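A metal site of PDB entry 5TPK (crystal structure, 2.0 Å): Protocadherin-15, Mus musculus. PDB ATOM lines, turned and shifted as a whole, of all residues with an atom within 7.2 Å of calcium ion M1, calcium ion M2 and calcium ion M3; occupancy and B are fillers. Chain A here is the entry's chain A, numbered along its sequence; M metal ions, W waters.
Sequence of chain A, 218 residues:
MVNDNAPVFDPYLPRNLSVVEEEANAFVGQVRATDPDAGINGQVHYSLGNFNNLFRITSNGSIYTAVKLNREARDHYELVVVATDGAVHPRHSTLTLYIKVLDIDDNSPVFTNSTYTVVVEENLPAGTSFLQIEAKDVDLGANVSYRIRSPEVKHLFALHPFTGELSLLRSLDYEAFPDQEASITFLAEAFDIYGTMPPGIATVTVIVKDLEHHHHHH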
ATOM      1  N   GLU A  21     -16.825 -18.671  29.946  1.00  0.00           N
ATOM      2  CA  GLU A  21     -15.971 -18.640  28.776  1.00  0.00           C
ATOM      3  C   GLU A  21     -15.850 -17.207  28.179  1.00  0.00           C
ATOM      4  O   GLU A  21     -16.658 -16.320  28.473  1.00  0.00           O
ATOM      5  CB  GLU A  21     -16.477 -19.584  27.686  1.00  0.00           C
ATOM      6  CG  GLU A  21     -17.821 -19.227  27.075  1.00  0.00           C
ATOM      7  CD  GLU A  21     -18.139 -20.005  25.820  1.00  0.00           C
ATOM      8  OE1 GLU A  21     -19.349 -20.217  25.569  1.00  0.00           O
ATOM      9  OE2 GLU A  21     -17.218 -20.379  25.063  1.00  0.00           O
ATOM     10  N   GLU A  22     -14.843 -17.049  27.315  1.00  0.00           N
ATOM     11  CA  GLU A  22     -14.660 -15.876  26.461  1.00  0.00           C
ATOM     12  C   GLU A  22     -14.378 -14.574  27.235  1.00  0.00           C
ATOM     13  O   GLU A  22     -14.808 -13.507  26.822  1.00  0.00           O
ATOM     14  CB  GLU A  22     -15.827 -15.705  25.480  1.00  0.00           C
ATOM     15  CG  GLU A  22     -16.150 -16.951  24.627  1.00  0.00           C
ATOM     16  CD  GLU A  22     -15.028 -17.382  23.670  1.00  0.00           C
ATOM     17  OE1 GLU A  22     -13.978 -16.719  23.559  1.00  0.00           O
ATOM     18  OE2 GLU A  22     -15.205 -18.427  23.003  1.00  0.00           O
ATOM     19  N   LEU A  69     -11.118 -18.283  27.607  1.00  0.00           N
ATOM     20  CA  LEU A  69     -11.345 -19.735  27.473  1.00  0.00           C
ATOM     21  C   LEU A  69     -12.493 -19.944  26.491  1.00  0.00           C
ATOM     22  O   LEU A  69     -13.413 -19.146  26.423  1.00  0.00           O
ATOM     23  CB  LEU A  69     -11.657 -20.387  28.812  1.00  0.00           C
ATOM     24  CG  LEU A  69     -10.608 -20.147  29.914  1.00  0.00           C
ATOM     25  CD1 LEU A  69     -11.048 -20.784  31.216  1.00  0.00           C
ATOM     26  CD2 LEU A  69      -9.231 -20.672  29.508  1.00  0.00           C
ATOM     27  N   ASN A  70     -12.430 -21.030  25.725  1.00  0.00           N
ATOM     28  CA  ASN A  70     -13.484 -21.357  24.784  1.00  0.00           C
ATOM     29  C   ASN A  70     -14.103 -22.680  25.218  1.00  0.00           C
ATOM     30  O   ASN A  70     -13.511 -23.750  25.047  1.00  0.00           O
ATOM     31  CB  ASN A  70     -12.914 -21.446  23.361  1.00  0.00           C
ATOM     32  CG  ASN A  70     -13.981 -21.727  22.315  1.00  0.00           C
ATOM     33  OD1 ASN A  70     -15.184 -21.634  22.581  1.00  0.00           O
ATOM     34  ND2 ASN A  70     -13.546 -22.060  21.117  1.00  0.00           N
ATOM     35  N   ARG A  71     -15.315 -22.596  25.762  1.00  0.00           N
ATOM     36  CA  ARG A  71     -16.032 -23.801  26.207  1.00  0.00           C
ATOM     37  C   ARG A  71     -16.200 -24.826  25.089  1.00  0.00           C
ATOM     38  O   ARG A  71     -16.149 -26.039  25.329  1.00  0.00           O
ATOM     39  CB  ARG A  71     -17.383 -23.460  26.805  1.00  0.00           C
ATOM     40  CG  ARG A  71     -17.939 -24.603  27.638  1.00  0.00           C
ATOM     41  CD  ARG A  71     -19.428 -24.777  27.483  1.00  0.00           C
ATOM     42  NE  ARG A  71     -19.910 -24.829  26.082  1.00  0.00           N
ATOM     43  CZ  ARG A  71     -20.089 -25.908  25.321  1.00  0.00           C
ATOM     44  NH1 ARG A  71     -20.564 -25.771  24.072  1.00  0.00           N
ATOM     45  NH2 ARG A  71     -19.823 -27.120  25.780  1.00  0.00           N
ATOM     46  N   GLU A  72     -16.418 -24.342  23.872  1.00  0.00           N
ATOM     47  CA  GLU A  72     -16.608 -25.201  22.707  1.00  0.00           C
ATOM     48  C   GLU A  72     -15.333 -26.007  22.395  1.00  0.00           C
ATOM     49  O   GLU A  72     -15.417 -27.042  21.764  1.00  0.00           O
ATOM     50  CB  GLU A  72     -17.068 -24.390  21.480  1.00  0.00           C
ATOM     51  CG  GLU A  72     -18.564 -24.066  21.437  1.00  0.00           C
ATOM     52  CD  GLU A  72     -19.018 -23.031  22.457  1.00  0.00           C
ATOM     53  OE1 GLU A  72     -18.442 -21.931  22.534  1.00  0.00           O
ATOM     54  OE2 GLU A  72     -20.022 -23.280  23.170  1.00  0.00           O
ATOM     55  N   ALA A  73     -14.162 -25.523  22.842  1.00  0.00           N
ATOM     56  CA  ALA A  73     -12.897 -26.236  22.652  1.00  0.00           C
ATOM     57  C   ALA A  73     -12.554 -27.112  23.853  1.00  0.00           C
ATOM     58  O   ALA A  73     -12.114 -28.243  23.676  1.00  0.00           O
ATOM     59  CB  ALA A  73     -11.764 -25.253  22.369  1.00  0.00           C
ATOM     60  N   LEU A 102     -17.991 -22.230  31.943  1.00  0.00           N
ATOM     61  CA  LEU A 102     -19.417 -22.076  31.736  1.00  0.00           C
ATOM     62  C   LEU A 102     -19.724 -21.536  30.345  1.00  0.00           C
ATOM     63  O   LEU A 102     -18.966 -20.734  29.826  1.00  0.00           O
ATOM     64  CB  LEU A 102     -19.978 -21.121  32.789  1.00  0.00           C
ATOM     65  CG  LEU A 102     -19.896 -21.649  34.216  1.00  0.00           C
ATOM     66  CD1 LEU A 102     -20.179 -20.519  35.192  1.00  0.00           C
ATOM     67  CD2 LEU A 102     -20.865 -22.813  34.394  1.00  0.00           C
ATOM     68  N   ASP A 103     -20.840 -21.983  29.787  1.00  0.00           N
ATOM     69  CA  ASP A 103     -21.238 -21.646  28.417  1.00  0.00           C
ATOM     70  C   ASP A 103     -21.915 -20.299  28.341  1.00  0.00           C
ATOM     71  O   ASP A 103     -22.703 -19.971  29.229  1.00  0.00           O
ATOM     72  CB  ASP A 103     -22.255 -22.667  27.892  1.00  0.00           C
ATOM     73  CG  ASP A 103     -22.440 -22.603  26.379  1.00  0.00           C
ATOM     74  OD1 ASP A 103     -21.423 -22.633  25.660  1.00  0.00           O
ATOM     75  OD2 ASP A 103     -23.586 -22.570  25.920  1.00  0.00           O
ATOM     76  N   ILE A 104     -21.635 -19.548  27.277  1.00  0.00           N
ATOM     77  CA  ILE A 104     -22.470 -18.434  26.829  1.00  0.00           C
ATOM     78  C   ILE A 104     -22.907 -18.712  25.407  1.00  0.00           C
ATOM     79  O   ILE A 104     -22.267 -19.460  24.679  1.00  0.00           O
ATOM     80  CB  ILE A 104     -21.751 -17.052  26.877  1.00  0.00           C
ATOM     81  CG1 ILE A 104     -20.648 -16.951  25.795  1.00  0.00           C
ATOM     82  CG2 ILE A 104     -21.156 -16.827  28.259  1.00  0.00           C
ATOM     83  CD1 ILE A 104     -19.968 -15.598  25.707  1.00  0.00           C
ATOM     84  N   ASP A 105     -24.007 -18.080  24.995  1.00  0.00           N
ATOM     85  CA  ASP A 105     -24.422 -18.112  23.604  1.00  0.00           C
ATOM     86  C   ASP A 105     -23.548 -17.184  22.769  1.00  0.00           C
ATOM     87  O   ASP A 105     -23.818 -16.005  22.658  1.00  0.00           O
ATOM     88  CB  ASP A 105     -25.893 -17.718  23.453  1.00  0.00           C
ATOM     89  CG  ASP A 105     -26.390 -17.840  22.021  1.00  0.00           C
ATOM     90  OD1 ASP A 105     -25.677 -18.430  21.172  1.00  0.00           O
ATOM     91  OD2 ASP A 105     -27.494 -17.344  21.741  1.00  0.00           O
ATOM     92  N   ASP A 106     -22.485 -17.741  22.201  1.00  0.00           N
ATOM     93  CA  ASP A 106     -21.562 -16.974  21.340  1.00  0.00           C
ATOM     94  C   ASP A 106     -21.442 -17.581  19.945  1.00  0.00           C
ATOM     95  O   ASP A 106     -20.560 -17.189  19.200  1.00  0.00           O
ATOM     96  CB  ASP A 106     -20.186 -16.809  22.008  1.00  0.00           C
ATOM     97  CG  ASP A 106     -19.494 -18.140  22.317  1.00  0.00           C
ATOM     98  OD1 ASP A 106     -20.169 -19.181  22.494  1.00  0.00           O
ATOM     99  OD2 ASP A 106     -18.245 -18.151  22.402  1.00  0.00           O
ATOM    100  N   ASN A 107     -22.331 -18.519  19.597  1.00  0.00           N
ATOM    101  CA  ASN A 107     -22.391 -19.056  18.241  1.00  0.00           C
ATOM    102  C   ASN A 107     -23.826 -19.038  17.714  1.00  0.00           C
ATOM    103  O   ASN A 107     -24.740 -19.539  18.369  1.00  0.00           O
ATOM    104  CB  ASN A 107     -21.878 -20.481  18.177  1.00  0.00           C
ATOM    105  CG  ASN A 107     -20.453 -20.603  18.627  1.00  0.00           C
ATOM    106  OD1 ASN A 107     -19.522 -20.543  17.810  1.00  0.00           O
ATOM    107  ND2 ASN A 107     -20.254 -20.773  19.932  1.00  0.00           N
ATOM    108  N   SER A 108     -24.000 -18.453  16.553  1.00  0.00           N
ATOM    109  CA  SER A 108     -25.247 -18.583  15.802  1.00  0.00           C
ATOM    110  C   SER A 108     -25.330 -19.960  15.174  1.00  0.00           C
ATOM    111  O   SER A 108     -24.289 -20.546  14.865  1.00  0.00           O
ATOM    112  CB  SER A 108     -25.309 -17.549  14.686  1.00  0.00           C
ATOM    113  OG  SER A 108     -25.380 -16.267  15.232  1.00  0.00           O
ATOM    114  N   PRO A 109     -26.551 -20.477  14.979  1.00  0.00           N
ATOM    115  CA  PRO A 109     -26.664 -21.684  14.176  1.00  0.00           C
ATOM    116  C   PRO A 109     -25.976 -21.503  12.821  1.00  0.00           C
ATOM    117  O   PRO A 109     -26.021 -20.416  12.285  1.00  0.00           O
ATOM    118  CB  PRO A 109     -28.188 -21.883  14.024  1.00  0.00           C
ATOM    119  CG  PRO A 109     -28.765 -21.198  15.196  1.00  0.00           C
ATOM    120  CD  PRO A 109     -27.866 -20.047  15.505  1.00  0.00           C
ATOM    121  N   LYS A 136     -26.689 -26.230  12.621  1.00  0.00           N
ATOM    122  CA  LYS A 136     -26.203 -26.739  13.915  1.00  0.00           C
ATOM    123  C   LYS A 136     -25.745 -25.573  14.771  1.00  0.00           C
ATOM    124  O   LYS A 136     -25.113 -24.642  14.272  1.00  0.00           O
ATOM    125  CB  LYS A 136     -25.074 -27.721  13.685  1.00  0.00           C
ATOM    126  CG  LYS A 136     -25.563 -29.045  13.115  1.00  0.00           C
ATOM    127  CD  LYS A 136     -24.413 -29.889  12.545  1.00  0.00           C
ATOM    128  CE  LYS A 136     -24.888 -30.751  11.377  1.00  0.00           C
ATOM    129  NZ  LYS A 136     -23.722 -31.360  10.677  1.00  0.00           N
ATOM    130  N   ASP A 137     -26.101 -25.614  16.048  1.00  0.00           N
ATOM    131  CA  ASP A 137     -25.641 -24.648  17.018  1.00  0.00           C
ATOM    132  C   ASP A 137     -24.726 -25.331  18.024  1.00  0.00           C
ATOM    133  O   ASP A 137     -25.165 -26.167  18.804  1.00  0.00           O
ATOM    134  CB  ASP A 137     -26.853 -24.040  17.721  1.00  0.00           C
ATOM    135  CG  ASP A 137     -26.515 -22.795  18.499  1.00  0.00           C
ATOM    136  OD1 ASP A 137     -25.468 -22.770  19.212  1.00  0.00           O
ATOM    137  OD2 ASP A 137     -27.289 -21.814  18.426  1.00  0.00           O
ATOM    138  N   VAL A 138     -23.452 -24.938  18.021  1.00  0.00           N
ATOM    139  CA  VAL A 138     -22.429 -25.560  18.884  1.00  0.00           C
ATOM    140  C   VAL A 138     -22.536 -25.234  20.389  1.00  0.00           C
ATOM    141  O   VAL A 138     -21.869 -25.864  21.210  1.00  0.00           O
ATOM    142  CB  VAL A 138     -20.989 -25.286  18.383  1.00  0.00           C
ATOM    143  CG1 VAL A 138     -20.807 -25.836  16.963  1.00  0.00           C
ATOM    144  CG2 VAL A 138     -20.625 -23.813  18.429  1.00  0.00           C
ATOM    145  N   ASP A 139     -23.358 -24.254  20.758  1.00  0.00           N
ATOM    146  CA  ASP A 139     -23.524 -23.885  22.178  1.00  0.00           C
ATOM    147  C   ASP A 139     -24.334 -24.926  22.924  1.00  0.00           C
ATOM    148  O   ASP A 139     -25.038 -25.733  22.335  1.00  0.00           O
ATOM    149  CB  ASP A 139     -24.179 -22.522  22.329  1.00  0.00           C
ATOM    150  CG  ASP A 139     -23.330 -21.402  21.748  1.00  0.00           C
ATOM    151  OD1 ASP A 139     -22.128 -21.298  22.103  1.00  0.00           O
ATOM    152  OD2 ASP A 139     -23.856 -20.632  20.922  1.00  0.00           O
ATOM    153  N   LEU A 140     -24.217 -24.873  24.246  1.00  0.00           N
ATOM    154  CA  LEU A 140     -24.802 -25.871  25.142  1.00  0.00           C
ATOM    155  C   LEU A 140     -26.329 -25.716  25.252  1.00  0.00           C
ATOM    156  O   LEU A 140     -26.830 -24.636  25.494  1.00  0.00           O
ATOM    157  CB  LEU A 140     -24.152 -25.724  26.533  1.00  0.00           C
ATOM    158  CG  LEU A 140     -24.149 -26.898  27.499  1.00  0.00           C
ATOM    159  CD1 LEU A 140     -23.440 -28.090  26.884  1.00  0.00           C
ATOM    160  CD2 LEU A 140     -23.454 -26.477  28.779  1.00  0.00           C
ATOM    161  N   ALA A 142     -28.674 -25.783  23.015  1.00  0.00           N
ATOM    162  CA  ALA A 142     -29.319 -24.989  21.989  1.00  0.00           C
ATOM    163  C   ALA A 142     -30.378 -25.867  21.310  1.00  0.00           C
ATOM    164  O   ALA A 142     -30.188 -27.069  21.179  1.00  0.00           O
ATOM    165  CB  ALA A 142     -28.296 -24.503  20.995  1.00  0.00           C
ATOM    166  N   ASP A 192     -31.690 -20.189  17.687  1.00  0.00           N
ATOM    167  CA  ASP A 192     -31.824 -20.804  19.005  1.00  0.00           C
ATOM    168  C   ASP A 192     -33.013 -20.134  19.675  1.00  0.00           C
ATOM    169  O   ASP A 192     -33.014 -18.928  19.925  1.00  0.00           O
ATOM    170  CB  ASP A 192     -30.554 -20.658  19.868  1.00  0.00           C
ATOM    171  CG  ASP A 192     -30.586 -21.519  21.146  1.00  0.00           C
ATOM    172  OD1 ASP A 192     -31.629 -22.143  21.455  1.00  0.00           O
ATOM    173  OD2 ASP A 192     -29.547 -21.564  21.858  1.00  0.00           O
ATOM    174  N   GLY A 195     -31.810 -18.573  22.730  1.00  0.00           N
ATOM    175  CA  GLY A 195     -30.514 -17.917  22.578  1.00  0.00           C
ATOM    176  C   GLY A 195     -30.650 -16.430  22.305  1.00  0.00           C
ATOM    177  O   GLY A 195     -31.761 -15.922  22.129  1.00  0.00           O
ATOM    178  N   THR A 196     -29.509 -15.744  22.282  1.00  0.00           N
ATOM    179  CA  THR A 196     -29.424 -14.313  22.053  1.00  0.00           C
ATOM    180  C   THR A 196     -28.612 -13.906  20.823  1.00  0.00           C
ATOM    181  O   THR A 196     -28.632 -12.723  20.446  1.00  0.00           O
ATOM    182  CB  THR A 196     -28.767 -13.630  23.262  1.00  0.00           C
ATOM    183  OG1 THR A 196     -27.471 -14.204  23.503  1.00  0.00           O
ATOM    184  CG2 THR A 196     -29.637 -13.781  24.506  1.00  0.00           C
ATOM    185  N   MET A 197     -27.878 -14.837  20.223  1.00  0.00           N
ATOM    186  CA  MET A 197     -27.093 -14.534  19.025  1.00  0.00           C
ATOM    187  C   MET A 197     -28.049 -14.335  17.845  1.00  0.00           C
ATOM    188  O   MET A 197     -29.214 -14.742  17.915  1.00  0.00           O
ATOM    189  CB  MET A 197     -26.100 -15.670  18.714  1.00  0.00           C
ATOM    190  CG  MET A 197     -24.826 -15.616  19.542  1.00  0.00           C
ATOM    191  SD  MET A 197     -23.673 -14.347  18.991  1.00  0.00           S
ATOM    192  CE  MET A 197     -22.863 -15.140  17.603  1.00  0.00           C
ATOM    193  N   PRO A 198     -27.555 -13.715  16.750  1.00  0.00           N
ATOM    194  CA  PRO A 198     -28.392 -13.608  15.550  1.00  0.00           C
ATOM    195  C   PRO A 198     -28.742 -14.983  14.967  1.00  0.00           C
ATOM    196  O   PRO A 198     -28.054 -15.964  15.266  1.00  0.00           O
ATOM    197  CB  PRO A 198     -27.519 -12.812  14.564  1.00  0.00           C
ATOM    198  CG  PRO A 198     -26.472 -12.163  15.396  1.00  0.00           C
ATOM    199  CD  PRO A 198     -26.246 -13.067  16.565  1.00  0.00           C
HETATM  200 CA    CA M   1     -16.949 -20.150  22.722  1.00  0.00          CA
HETATM  201 CA    CA M   2     -20.716 -21.053  23.897  1.00  0.00          CA
HETATM  202 CA    CA M   3     -26.009 -20.404  19.991  1.00  0.00          CA
HETATM  203  O   HOH W   1     -27.890 -18.961  19.446  1.00  0.00           O
HETATM  204  O   HOH W   2     -27.141 -20.916  21.660  1.00  0.00           O
HETATM  205  O   HOH W   3     -17.035 -20.114  20.372  1.00  0.00           O
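Of the 26 residues printed, 4 come within 4 Å of calcium ion M3.
Within 4 Å of calcium ion M1: Glu 21, Glu 22, Asn 70, Glu 72 and Asp 106. The nearest printed residue that does not touch calcium ion M1 is Arg 71 (4.2 Å).
The side-chain carboxylate (OE2) of Glu 72 sits close to the guanidinium group (NH1) of Arg 71 (2.7 Å). N of Arg 71 lies close to OE2 of Glu 21 (3.0 Å). The side-chain carboxylate (OD2) of Asp 105 is in hydrogen-bond range of the backbone NH (N) of Thr 196 (2.6 Å). The side-chain carboxylate (OD1) of Asp 103 lies close to the guanidinium group (NE) of Arg 71, 2.7 Å away. N of Glu 22 is in hydrogen-bond range of O of Leu 69. OD2 of Asp 103 sits at hydrogen-bond distance from N of Leu 140. OE1 of Glu 72 lies close to ND2 of Asn 107, 3.4 Å away. The side-chain carboxylate (OD2) of Asp 105 is in hydrogen-bond range of the backbone NH (N) of Met 197, 3.0 Å away.
Calcium ion M3 is bound by water W2, O of Asn 107, OD1 of Asp 105, OD2 of Asp 139, water W1, OD2 of Asp 137 and OD1 of Asp 137. Calcium ion M3 has seven donor atoms within binding distance.
Calcium ion M2 is bound by OD1 of Asp 139, 2.3 Å away. OE1 of Glu 21 is bound to calcium ion M2, 2.3 Å away. Calcium ion M2 is bound by O of Ile 104 (2.4 Å). OD1 of Asp 106 is bound to calcium ion M2 (2.4 Å). OE2 of Glu 72 binds calcium ion M2, 2.4 Å away. OD1 of Asp 103 is bound to calcium ion M2, at 2.5 Å. The side-chain carboxylate (OE1) of Glu 72 binds calcium ion M2 (2.8 Å). Calcium ion M2 has seven donor atoms within binding distance.
The side-chain amide oxygen (OD1) of Asn 70 is bound to calcium ion M1, at 2.3 Å. The side-chain carboxylate (OE1) of Glu 72 is bound to calcium ion M1 (2.3 Å). Calcium ion M1 is bound by water W3 (2.4 Å). Calcium ion M1 is bound by OE2 of Glu 21, 2.4 Å away. OD2 of Asp 106 binds calcium ion M1, at 2.4 Å. Calcium ion M1 is bound by the side-chain carboxylate (OE2) of Glu 22, at 2.5 Å. Calcium ion M1 has six donor atoms within binding distance.
The nearest printed residue that does not touch calcium ion M2 is Asn 107 (4.002 Å).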
